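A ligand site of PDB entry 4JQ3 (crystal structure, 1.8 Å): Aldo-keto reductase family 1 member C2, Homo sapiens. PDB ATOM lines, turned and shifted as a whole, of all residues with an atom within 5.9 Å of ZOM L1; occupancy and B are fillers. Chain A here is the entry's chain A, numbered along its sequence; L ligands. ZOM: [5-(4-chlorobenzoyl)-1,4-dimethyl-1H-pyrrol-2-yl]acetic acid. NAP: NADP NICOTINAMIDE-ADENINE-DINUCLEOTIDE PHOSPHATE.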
ATOM      1  N   TYR A  24      -1.653  12.987 -14.950  1.00  0.00           N
ATOM      2  CA  TYR A  24      -1.961  12.257 -16.181  1.00  0.00           C
ATOM      3  C   TYR A  24      -1.989  10.750 -15.972  1.00  0.00           C
ATOM      4  O   TYR A  24      -1.074  10.201 -15.336  1.00  0.00           O
ATOM      5  CB  TYR A  24      -0.947  12.515 -17.249  1.00  0.00           C
ATOM      6  CG  TYR A  24      -1.272  11.642 -18.427  1.00  0.00           C
ATOM      7  CD1 TYR A  24      -2.493  11.772 -19.119  1.00  0.00           C
ATOM      8  CD2 TYR A  24      -0.405  10.611 -18.798  1.00  0.00           C
ATOM      9  CE1 TYR A  24      -2.825  10.913 -20.162  1.00  0.00           C
ATOM     10  CE2 TYR A  24      -0.712   9.758 -19.863  1.00  0.00           C
ATOM     11  CZ  TYR A  24      -1.928   9.913 -20.530  1.00  0.00           C
ATOM     12  OH  TYR A  24      -2.210   9.043 -21.562  1.00  0.00           O
ATOM     13  N   ALA A  52      -3.854  19.658 -16.734  1.00  0.00           N
ATOM     14  CA  ALA A  52      -3.881  20.221 -18.102  1.00  0.00           C
ATOM     15  C   ALA A  52      -5.233  19.931 -18.716  1.00  0.00           C
ATOM     16  O   ALA A  52      -5.864  18.906 -18.435  1.00  0.00           O
ATOM     17  CB  ALA A  52      -2.824  19.591 -18.984  1.00  0.00           C
ATOM     18  N   VAL A  54      -5.755  18.841 -21.657  1.00  0.00           N
ATOM     19  CA  VAL A  54      -5.668  17.713 -22.585  1.00  0.00           C
ATOM     20  C   VAL A  54      -5.737  16.397 -21.799  1.00  0.00           C
ATOM     21  O   VAL A  54      -6.120  15.390 -22.335  1.00  0.00           O
ATOM     22  CB  VAL A  54      -4.398  17.956 -23.477  1.00  0.00           C
ATOM     23  CG1 VAL A  54      -3.126  17.398 -22.861  1.00  0.00           C
ATOM     24  CG2 VAL A  54      -4.609  17.543 -24.941  1.00  0.00           C
ATOM     25  N   TYR A  55      -5.477  16.407 -20.497  1.00  0.00           N
ATOM     26  CA  TYR A  55      -5.628  15.194 -19.643  1.00  0.00           C
ATOM     27  C   TYR A  55      -7.059  14.742 -19.390  1.00  0.00           C
ATOM     28  O   TYR A  55      -7.273  13.597 -18.980  1.00  0.00           O
ATOM     29  CB  TYR A  55      -4.944  15.329 -18.285  1.00  0.00           C
ATOM     30  CG  TYR A  55      -3.485  15.755 -18.322  1.00  0.00           C
ATOM     31  CD1 TYR A  55      -2.754  15.701 -19.479  1.00  0.00           C
ATOM     32  CD2 TYR A  55      -2.834  16.193 -17.161  1.00  0.00           C
ATOM     33  CE1 TYR A  55      -1.391  16.069 -19.517  1.00  0.00           C
ATOM     34  CE2 TYR A  55      -1.481  16.580 -17.187  1.00  0.00           C
ATOM     35  CZ  TYR A  55      -0.760  16.509 -18.376  1.00  0.00           C
ATOM     36  OH  TYR A  55       0.549  16.952 -18.395  1.00  0.00           O
ATOM     37  N   LYS A  84      -2.581  23.868 -18.295  1.00  0.00           N
ATOM     38  CA  LYS A  84      -1.820  24.049 -19.500  1.00  0.00           C
ATOM     39  C   LYS A  84      -2.771  24.334 -20.644  1.00  0.00           C
ATOM     40  O   LYS A  84      -3.839  23.732 -20.762  1.00  0.00           O
ATOM     41  CB  LYS A  84      -0.894  22.841 -19.786  1.00  0.00           C
ATOM     42  CG  LYS A  84      -0.019  22.455 -18.607  1.00  0.00           C
ATOM     43  CD  LYS A  84       0.981  21.325 -18.938  1.00  0.00           C
ATOM     44  CE  LYS A  84       1.598  20.652 -17.684  1.00  0.00           C
ATOM     45  NZ  LYS A  84       0.726  19.574 -17.109  1.00  0.00           N
ATOM     46  N   TRP A  86      -3.760  24.067 -24.215  1.00  0.00           N
ATOM     47  CA  TRP A  86      -3.566  23.058 -25.303  1.00  0.00           C
ATOM     48  C   TRP A  86      -3.385  23.772 -26.652  1.00  0.00           C
ATOM     49  O   TRP A  86      -3.789  24.930 -26.850  1.00  0.00           O
ATOM     50  CB  TRP A  86      -4.644  21.926 -25.340  1.00  0.00           C
ATOM     51  CG  TRP A  86      -4.207  20.858 -26.382  1.00  0.00           C
ATOM     52  CD1 TRP A  86      -4.876  20.481 -27.511  1.00  0.00           C
ATOM     53  CD2 TRP A  86      -2.912  20.231 -26.451  1.00  0.00           C
ATOM     54  NE1 TRP A  86      -4.081  19.647 -28.268  1.00  0.00           N
ATOM     55  CE2 TRP A  86      -2.881  19.457 -27.618  1.00  0.00           C
ATOM     56  CE3 TRP A  86      -1.771  20.222 -25.622  1.00  0.00           C
ATOM     57  CZ2 TRP A  86      -1.732  18.724 -27.999  1.00  0.00           C
ATOM     58  CZ3 TRP A  86      -0.676  19.513 -25.978  1.00  0.00           C
ATOM     59  CH2 TRP A  86      -0.641  18.773 -27.156  1.00  0.00           C
ATOM     60  N   HIS A 117       1.422  24.506 -23.334  1.00  0.00           N
ATOM     61  CA  HIS A 117       1.685  23.055 -23.163  1.00  0.00           C
ATOM     62  C   HIS A 117       2.708  22.520 -24.161  1.00  0.00           C
ATOM     63  O   HIS A 117       3.613  21.767 -23.779  1.00  0.00           O
ATOM     64  CB  HIS A 117       0.390  22.270 -23.247  1.00  0.00           C
ATOM     65  CG  HIS A 117       0.460  20.897 -22.667  1.00  0.00           C
ATOM     66  ND1 HIS A 117      -0.666  20.209 -22.266  1.00  0.00           N
ATOM     67  CD2 HIS A 117       1.517  20.112 -22.355  1.00  0.00           C
ATOM     68  CE1 HIS A 117      -0.319  19.052 -21.757  1.00  0.00           C
ATOM     69  NE2 HIS A 117       1.003  18.956 -21.816  1.00  0.00           N
ATOM     70  N   VAL A 128      -8.776  17.764 -29.564  1.00  0.00           N
ATOM     71  CA  VAL A 128      -7.418  18.010 -29.088  1.00  0.00           C
ATOM     72  C   VAL A 128      -6.361  17.735 -30.154  1.00  0.00           C
ATOM     73  O   VAL A 128      -5.375  18.505 -30.287  1.00  0.00           O
ATOM     74  CB  VAL A 128      -7.078  17.234 -27.793  1.00  0.00           C
ATOM     75  CG1 VAL A 128      -7.779  17.872 -26.614  1.00  0.00           C
ATOM     76  CG2 VAL A 128      -7.489  15.784 -27.889  1.00  0.00           C
ATOM     77  N   ILE A 129      -6.574  16.666 -30.936  1.00  0.00           N
ATOM     78  CA  ILE A 129      -5.710  16.312 -32.061  1.00  0.00           C
ATOM     79  C   ILE A 129      -6.614  16.289 -33.316  1.00  0.00           C
ATOM     80  O   ILE A 129      -7.092  15.257 -33.733  1.00  0.00           O
ATOM     81  CB  ILE A 129      -4.912  15.015 -31.810  1.00  0.00           C
ATOM     82  CG1 ILE A 129      -3.941  15.262 -30.619  1.00  0.00           C
ATOM     83  CG2 ILE A 129      -4.069  14.676 -33.021  1.00  0.00           C
ATOM     84  CD1 ILE A 129      -3.197  14.065 -30.122  1.00  0.00           C
ATOM     85  N   GLN A 190       8.600  23.406 -18.249  1.00  0.00           N
ATOM     86  CA  GLN A 190       8.316  22.056 -17.800  1.00  0.00           C
ATOM     87  C   GLN A 190       8.674  21.118 -18.942  1.00  0.00           C
ATOM     88  O   GLN A 190       8.062  21.177 -20.008  1.00  0.00           O
ATOM     89  CB  GLN A 190       6.827  21.906 -17.386  1.00  0.00           C
ATOM     90  CG  GLN A 190       6.513  20.485 -16.924  1.00  0.00           C
ATOM     91  CD  GLN A 190       5.055  20.198 -16.543  1.00  0.00           C
ATOM     92  OE1 GLN A 190       4.512  19.169 -16.936  1.00  0.00           O
ATOM     93  NE2 GLN A 190       4.467  21.024 -15.691  1.00  0.00           N
ATOM     94  N   HIS A 222       5.040   6.996 -17.757  1.00  0.00           N
ATOM     95  CA  HIS A 222       3.979   5.974 -17.968  1.00  0.00           C
ATOM     96  C   HIS A 222       4.438   4.688 -18.755  1.00  0.00           C
ATOM     97  O   HIS A 222       3.924   3.584 -18.515  1.00  0.00           O
ATOM     98  CB  HIS A 222       2.677   6.621 -18.577  1.00  0.00           C
ATOM     99  CG  HIS A 222       2.910   7.811 -19.501  1.00  0.00           C
ATOM    100  ND1 HIS A 222       3.129   7.676 -20.862  1.00  0.00           N
ATOM    101  CD2 HIS A 222       2.911   9.148 -19.258  1.00  0.00           C
ATOM    102  CE1 HIS A 222       3.269   8.877 -21.412  1.00  0.00           C
ATOM    103  NE2 HIS A 222       3.153   9.781 -20.456  1.00  0.00           N
ATOM    104  N   TRP A 227       3.145   6.326 -27.385  1.00  0.00           N
ATOM    105  CA  TRP A 227       3.981   7.525 -27.042  1.00  0.00           C
ATOM    106  C   TRP A 227       5.440   7.213 -26.642  1.00  0.00           C
ATOM    107  O   TRP A 227       6.345   8.048 -26.868  1.00  0.00           O
ATOM    108  CB  TRP A 227       3.351   8.401 -25.929  1.00  0.00           C
ATOM    109  CG  TRP A 227       1.909   8.711 -26.060  1.00  0.00           C
ATOM    110  CD1 TRP A 227       0.934   8.316 -25.209  1.00  0.00           C
ATOM    111  CD2 TRP A 227       1.256   9.474 -27.105  1.00  0.00           C
ATOM    112  NE1 TRP A 227      -0.272   8.767 -25.643  1.00  0.00           N
ATOM    113  CE2 TRP A 227      -0.112   9.476 -26.805  1.00  0.00           C
ATOM    114  CE3 TRP A 227       1.693  10.140 -28.252  1.00  0.00           C
ATOM    115  CZ2 TRP A 227      -1.069  10.135 -27.616  1.00  0.00           C
ATOM    116  CZ3 TRP A 227       0.742  10.805 -29.058  1.00  0.00           C
ATOM    117  CH2 TRP A 227      -0.613  10.779 -28.733  1.00  0.00           C
ATOM    118  N   LEU A 306       9.653  10.835 -24.320  1.00  0.00           N
ATOM    119  CA  LEU A 306       8.479  11.476 -24.856  1.00  0.00           C
ATOM    120  C   LEU A 306       8.839  12.388 -26.014  1.00  0.00           C
ATOM    121  O   LEU A 306       9.275  13.515 -25.825  1.00  0.00           O
ATOM    122  CB  LEU A 306       7.723  12.267 -23.777  1.00  0.00           C
ATOM    123  CG  LEU A 306       6.258  12.444 -24.203  1.00  0.00           C
ATOM    124  CD1 LEU A 306       5.527  11.104 -24.178  1.00  0.00           C
ATOM    125  CD2 LEU A 306       5.499  13.427 -23.321  1.00  0.00           C
ATOM    126  N   LEU A 308       6.535  12.913 -28.717  1.00  0.00           N
ATOM    127  CA  LEU A 308       5.358  13.449 -29.377  1.00  0.00           C
ATOM    128  C   LEU A 308       5.566  13.676 -30.891  1.00  0.00           C
ATOM    129  O   LEU A 308       5.293  14.780 -31.437  1.00  0.00           O
ATOM    130  CB  LEU A 308       4.999  14.773 -28.711  1.00  0.00           C
ATOM    131  CG  LEU A 308       3.542  15.155 -28.783  1.00  0.00           C
ATOM    132  CD1 LEU A 308       2.562  14.000 -29.111  1.00  0.00           C
ATOM    133  CD2 LEU A 308       3.211  15.835 -27.454  1.00  0.00           C
ATOM    134  N   PHE A 311       3.635  15.394 -33.818  1.00  0.00           N
ATOM    135  CA  PHE A 311       3.694  16.834 -34.073  1.00  0.00           C
ATOM    136  C   PHE A 311       4.979  17.310 -34.763  1.00  0.00           C
ATOM    137  O   PHE A 311       5.236  18.538 -34.882  1.00  0.00           O
ATOM    138  CB  PHE A 311       3.457  17.644 -32.804  1.00  0.00           C
ATOM    139  CG  PHE A 311       2.130  17.392 -32.171  1.00  0.00           C
ATOM    140  CD1 PHE A 311       0.976  17.519 -32.869  1.00  0.00           C
ATOM    141  CD2 PHE A 311       2.034  17.079 -30.850  1.00  0.00           C
ATOM    142  CE1 PHE A 311      -0.270  17.303 -32.302  1.00  0.00           C
ATOM    143  CE2 PHE A 311       0.794  16.837 -30.252  1.00  0.00           C
ATOM    144  CZ  PHE A 311      -0.366  16.961 -30.983  1.00  0.00           C
HETATM  145 CL   ZOM L   1      -6.370  12.353 -28.524  1.00  0.00          CL
HETATM  146  N1  ZOM L   1      -0.661  14.063 -23.061  1.00  0.00           N
HETATM  147  C2  ZOM L   1       0.380  14.862 -23.401  1.00  0.00           C
HETATM  148  C3  ZOM L   1       0.086  15.529 -24.503  1.00  0.00           C
HETATM  149  C4  ZOM L   1      -1.169  15.156 -24.825  1.00  0.00           C
HETATM  150  C5  ZOM L   1      -1.652  14.219 -23.943  1.00  0.00           C
HETATM  151  C6  ZOM L   1      -2.908  13.601 -23.833  1.00  0.00           C
HETATM  152  O6  ZOM L   1      -3.447  13.400 -22.735  1.00  0.00           O
HETATM  153  C7  ZOM L   1       1.722  14.962 -22.647  1.00  0.00           C
HETATM  154  C8  ZOM L   1       1.492  15.208 -21.149  1.00  0.00           C
HETATM  155  C9  ZOM L   1      -0.714  13.130 -21.894  1.00  0.00           C
HETATM  156  OH  ZOM L   1       1.371  16.401 -20.782  1.00  0.00           O
HETATM  157  C10 ZOM L   1      -1.867  15.753 -26.028  1.00  0.00           C
HETATM  158  C1B ZOM L   1      -3.711  13.297 -24.934  1.00  0.00           C
HETATM  159  C2B ZOM L   1      -5.115  13.487 -24.818  1.00  0.00           C
HETATM  160  C3B ZOM L   1      -5.962  13.197 -25.896  1.00  0.00           C
HETATM  161  C4B ZOM L   1      -5.372  12.719 -27.073  1.00  0.00           C
HETATM  162  C5B ZOM L   1      -3.992  12.532 -27.156  1.00  0.00           C
HETATM  163  C6B ZOM L   1      -3.155  12.814 -26.099  1.00  0.00           C
HETATM  164  OXT ZOM L   1       1.475  14.217 -20.365  1.00  0.00           O
HETATM  165  PA  NAP L   2       6.293   9.865 -13.909  1.00  0.00           P
HETATM  166  O1A NAP L   2       7.687   9.480 -14.268  1.00  0.00           O
HETATM  167  O2A NAP L   2       5.857  10.362 -12.496  1.00  0.00           O
HETATM  168  O5B NAP L   2       5.894   8.300 -13.358  1.00  0.00           O
HETATM  169  C5B NAP L   2       5.793   7.088 -14.074  1.00  0.00           C
HETATM  170  C4B NAP L   2       5.412   5.819 -13.181  1.00  0.00           C
HETATM  171  O4B NAP L   2       5.985   5.694 -11.877  1.00  0.00           O
HETATM  172  C3B NAP L   2       3.888   5.776 -12.902  1.00  0.00           C
HETATM  173  O3B NAP L   2       3.420   4.815 -13.763  1.00  0.00           O
HETATM  174  C2B NAP L   2       3.669   5.318 -11.426  1.00  0.00           C
HETATM  175  O2B NAP L   2       2.734   4.165 -11.268  1.00  0.00           O
HETATM  176  C1B NAP L   2       5.102   4.927 -11.008  1.00  0.00           C
HETATM  177  N9A NAP L   2       5.571   5.325  -9.617  1.00  0.00           N
HETATM  178  C8A NAP L   2       5.282   6.435  -8.900  1.00  0.00           C
HETATM  179  N7A NAP L   2       5.942   6.398  -7.749  1.00  0.00           N
HETATM  180  C5A NAP L   2       6.644   5.253  -7.727  1.00  0.00           C
HETATM  181  C6A NAP L   2       7.472   4.686  -6.803  1.00  0.00           C
HETATM  182  N6A NAP L   2       7.662   5.374  -5.659  1.00  0.00           N
HETATM  183  N1A NAP L   2       8.079   3.492  -7.019  1.00  0.00           N
HETATM  184  C2A NAP L   2       7.854   2.822  -8.206  1.00  0.00           C
HETATM  185  N3A NAP L   2       6.993   3.407  -9.155  1.00  0.00           N
HETATM  186  C4A NAP L   2       6.421   4.605  -8.905  1.00  0.00           C
HETATM  187  O3  NAP L   2       5.081   9.745 -15.083  1.00  0.00           O
HETATM  188  PN  NAP L   2       4.494  10.963 -16.181  1.00  0.00           P
HETATM  189  O1N NAP L   2       5.186  10.370 -17.269  1.00  0.00           O
HETATM  190  O2N NAP L   2       3.085  10.611 -15.754  1.00  0.00           O
HETATM  191  O5D NAP L   2       5.105  12.314 -15.521  1.00  0.00           O
HETATM  192  C5D NAP L   2       4.535  12.871 -14.326  1.00  0.00           C
HETATM  193  C4D NAP L   2       3.649  14.042 -14.632  1.00  0.00           C
HETATM  194  O4D NAP L   2       4.331  14.987 -15.478  1.00  0.00           O
HETATM  195  C3D NAP L   2       2.305  13.708 -15.384  1.00  0.00           C
HETATM  196  O3D NAP L   2       1.299  12.983 -14.581  1.00  0.00           O
HETATM  197  C2D NAP L   2       1.847  15.170 -15.800  1.00  0.00           C
HETATM  198  O2D NAP L   2       1.262  15.933 -14.730  1.00  0.00           O
HETATM  199  C1D NAP L   2       3.254  15.749 -16.185  1.00  0.00           C
HETATM  200  N1N NAP L   2       3.658  15.544 -17.612  1.00  0.00           N
HETATM  201  C2N NAP L   2       3.682  16.693 -18.407  1.00  0.00           C
HETATM  202  C3N NAP L   2       4.040  16.608 -19.750  1.00  0.00           C
HETATM  203  C7N NAP L   2       4.053  17.797 -20.542  1.00  0.00           C
HETATM  204  O7N NAP L   2       4.078  17.737 -21.759  1.00  0.00           O
HETATM  205  N7N NAP L   2       4.079  18.979 -19.905  1.00  0.00           N
HETATM  206  C4N NAP L   2       4.435  15.349 -20.258  1.00  0.00           C
HETATM  207  C5N NAP L   2       4.436  14.175 -19.487  1.00  0.00           C
HETATM  208  C6N NAP L   2       4.034  14.248 -18.153  1.00  0.00           C
HETATM  209  P2B NAP L   2       1.607   4.168 -10.108  1.00  0.00           P
HETATM  210  O1X NAP L   2       0.621   5.224 -10.514  1.00  0.00           O
HETATM  211  O2X NAP L   2       1.115   2.795 -10.168  1.00  0.00           O
HETATM  212  O3X NAP L   2       2.325   4.454  -8.819  1.00  0.00           O
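A ring nitrogen (NE2) of His 117 is in hydrogen-bond range of an oxygen (OH) of ZOM L1 (2.8 Å). The side-chain hydroxyl of Tyr 55 lies within hydrogen-bond range of an oxygen (OH) of ZOM L1 (2.6 Å). N of Tyr 24 sits at hydrogen-bond distance from O3D of NAP L2 (3.0 Å). The side-chain amide oxygen (OE1) of Gln 190 sits close to a nitrogen (N7N) of NAP L2, at 3.0 Å. An oxygen (O1N) of NAP L2 sits close to the backbone NH (N) of His 222. An oxygen (O7N) of NAP L2 sits at hydrogen-bond distance from a ring nitrogen (NE2) of His 117 (3.3 Å).
The side-chain hydroxyl (OH) of Tyr 55 is in hydrogen-bond range of the side-chain amino group (NZ) of Lys 84 (2.9 Å). The backbone carbonyl oxygen of Val 128 sits at hydrogen-bond distance from the indole nitrogen of Trp 86 (2.7 Å).
O of Val 54 lies close to O6 of ZOM L1 (3.4 Å). Residues that only touch ZOM L1: Ile 129, Trp 86, Tyr 24, Val 128 and Trp 227. Within 4 Å of ZOM L1: Tyr 24, Val 54, Tyr 55, Trp 86, His 117, Val 128, Ile 129 and Trp 227. The nearest printed residue that does not touch ZOM L1 is Leu 306 (4.1 Å).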
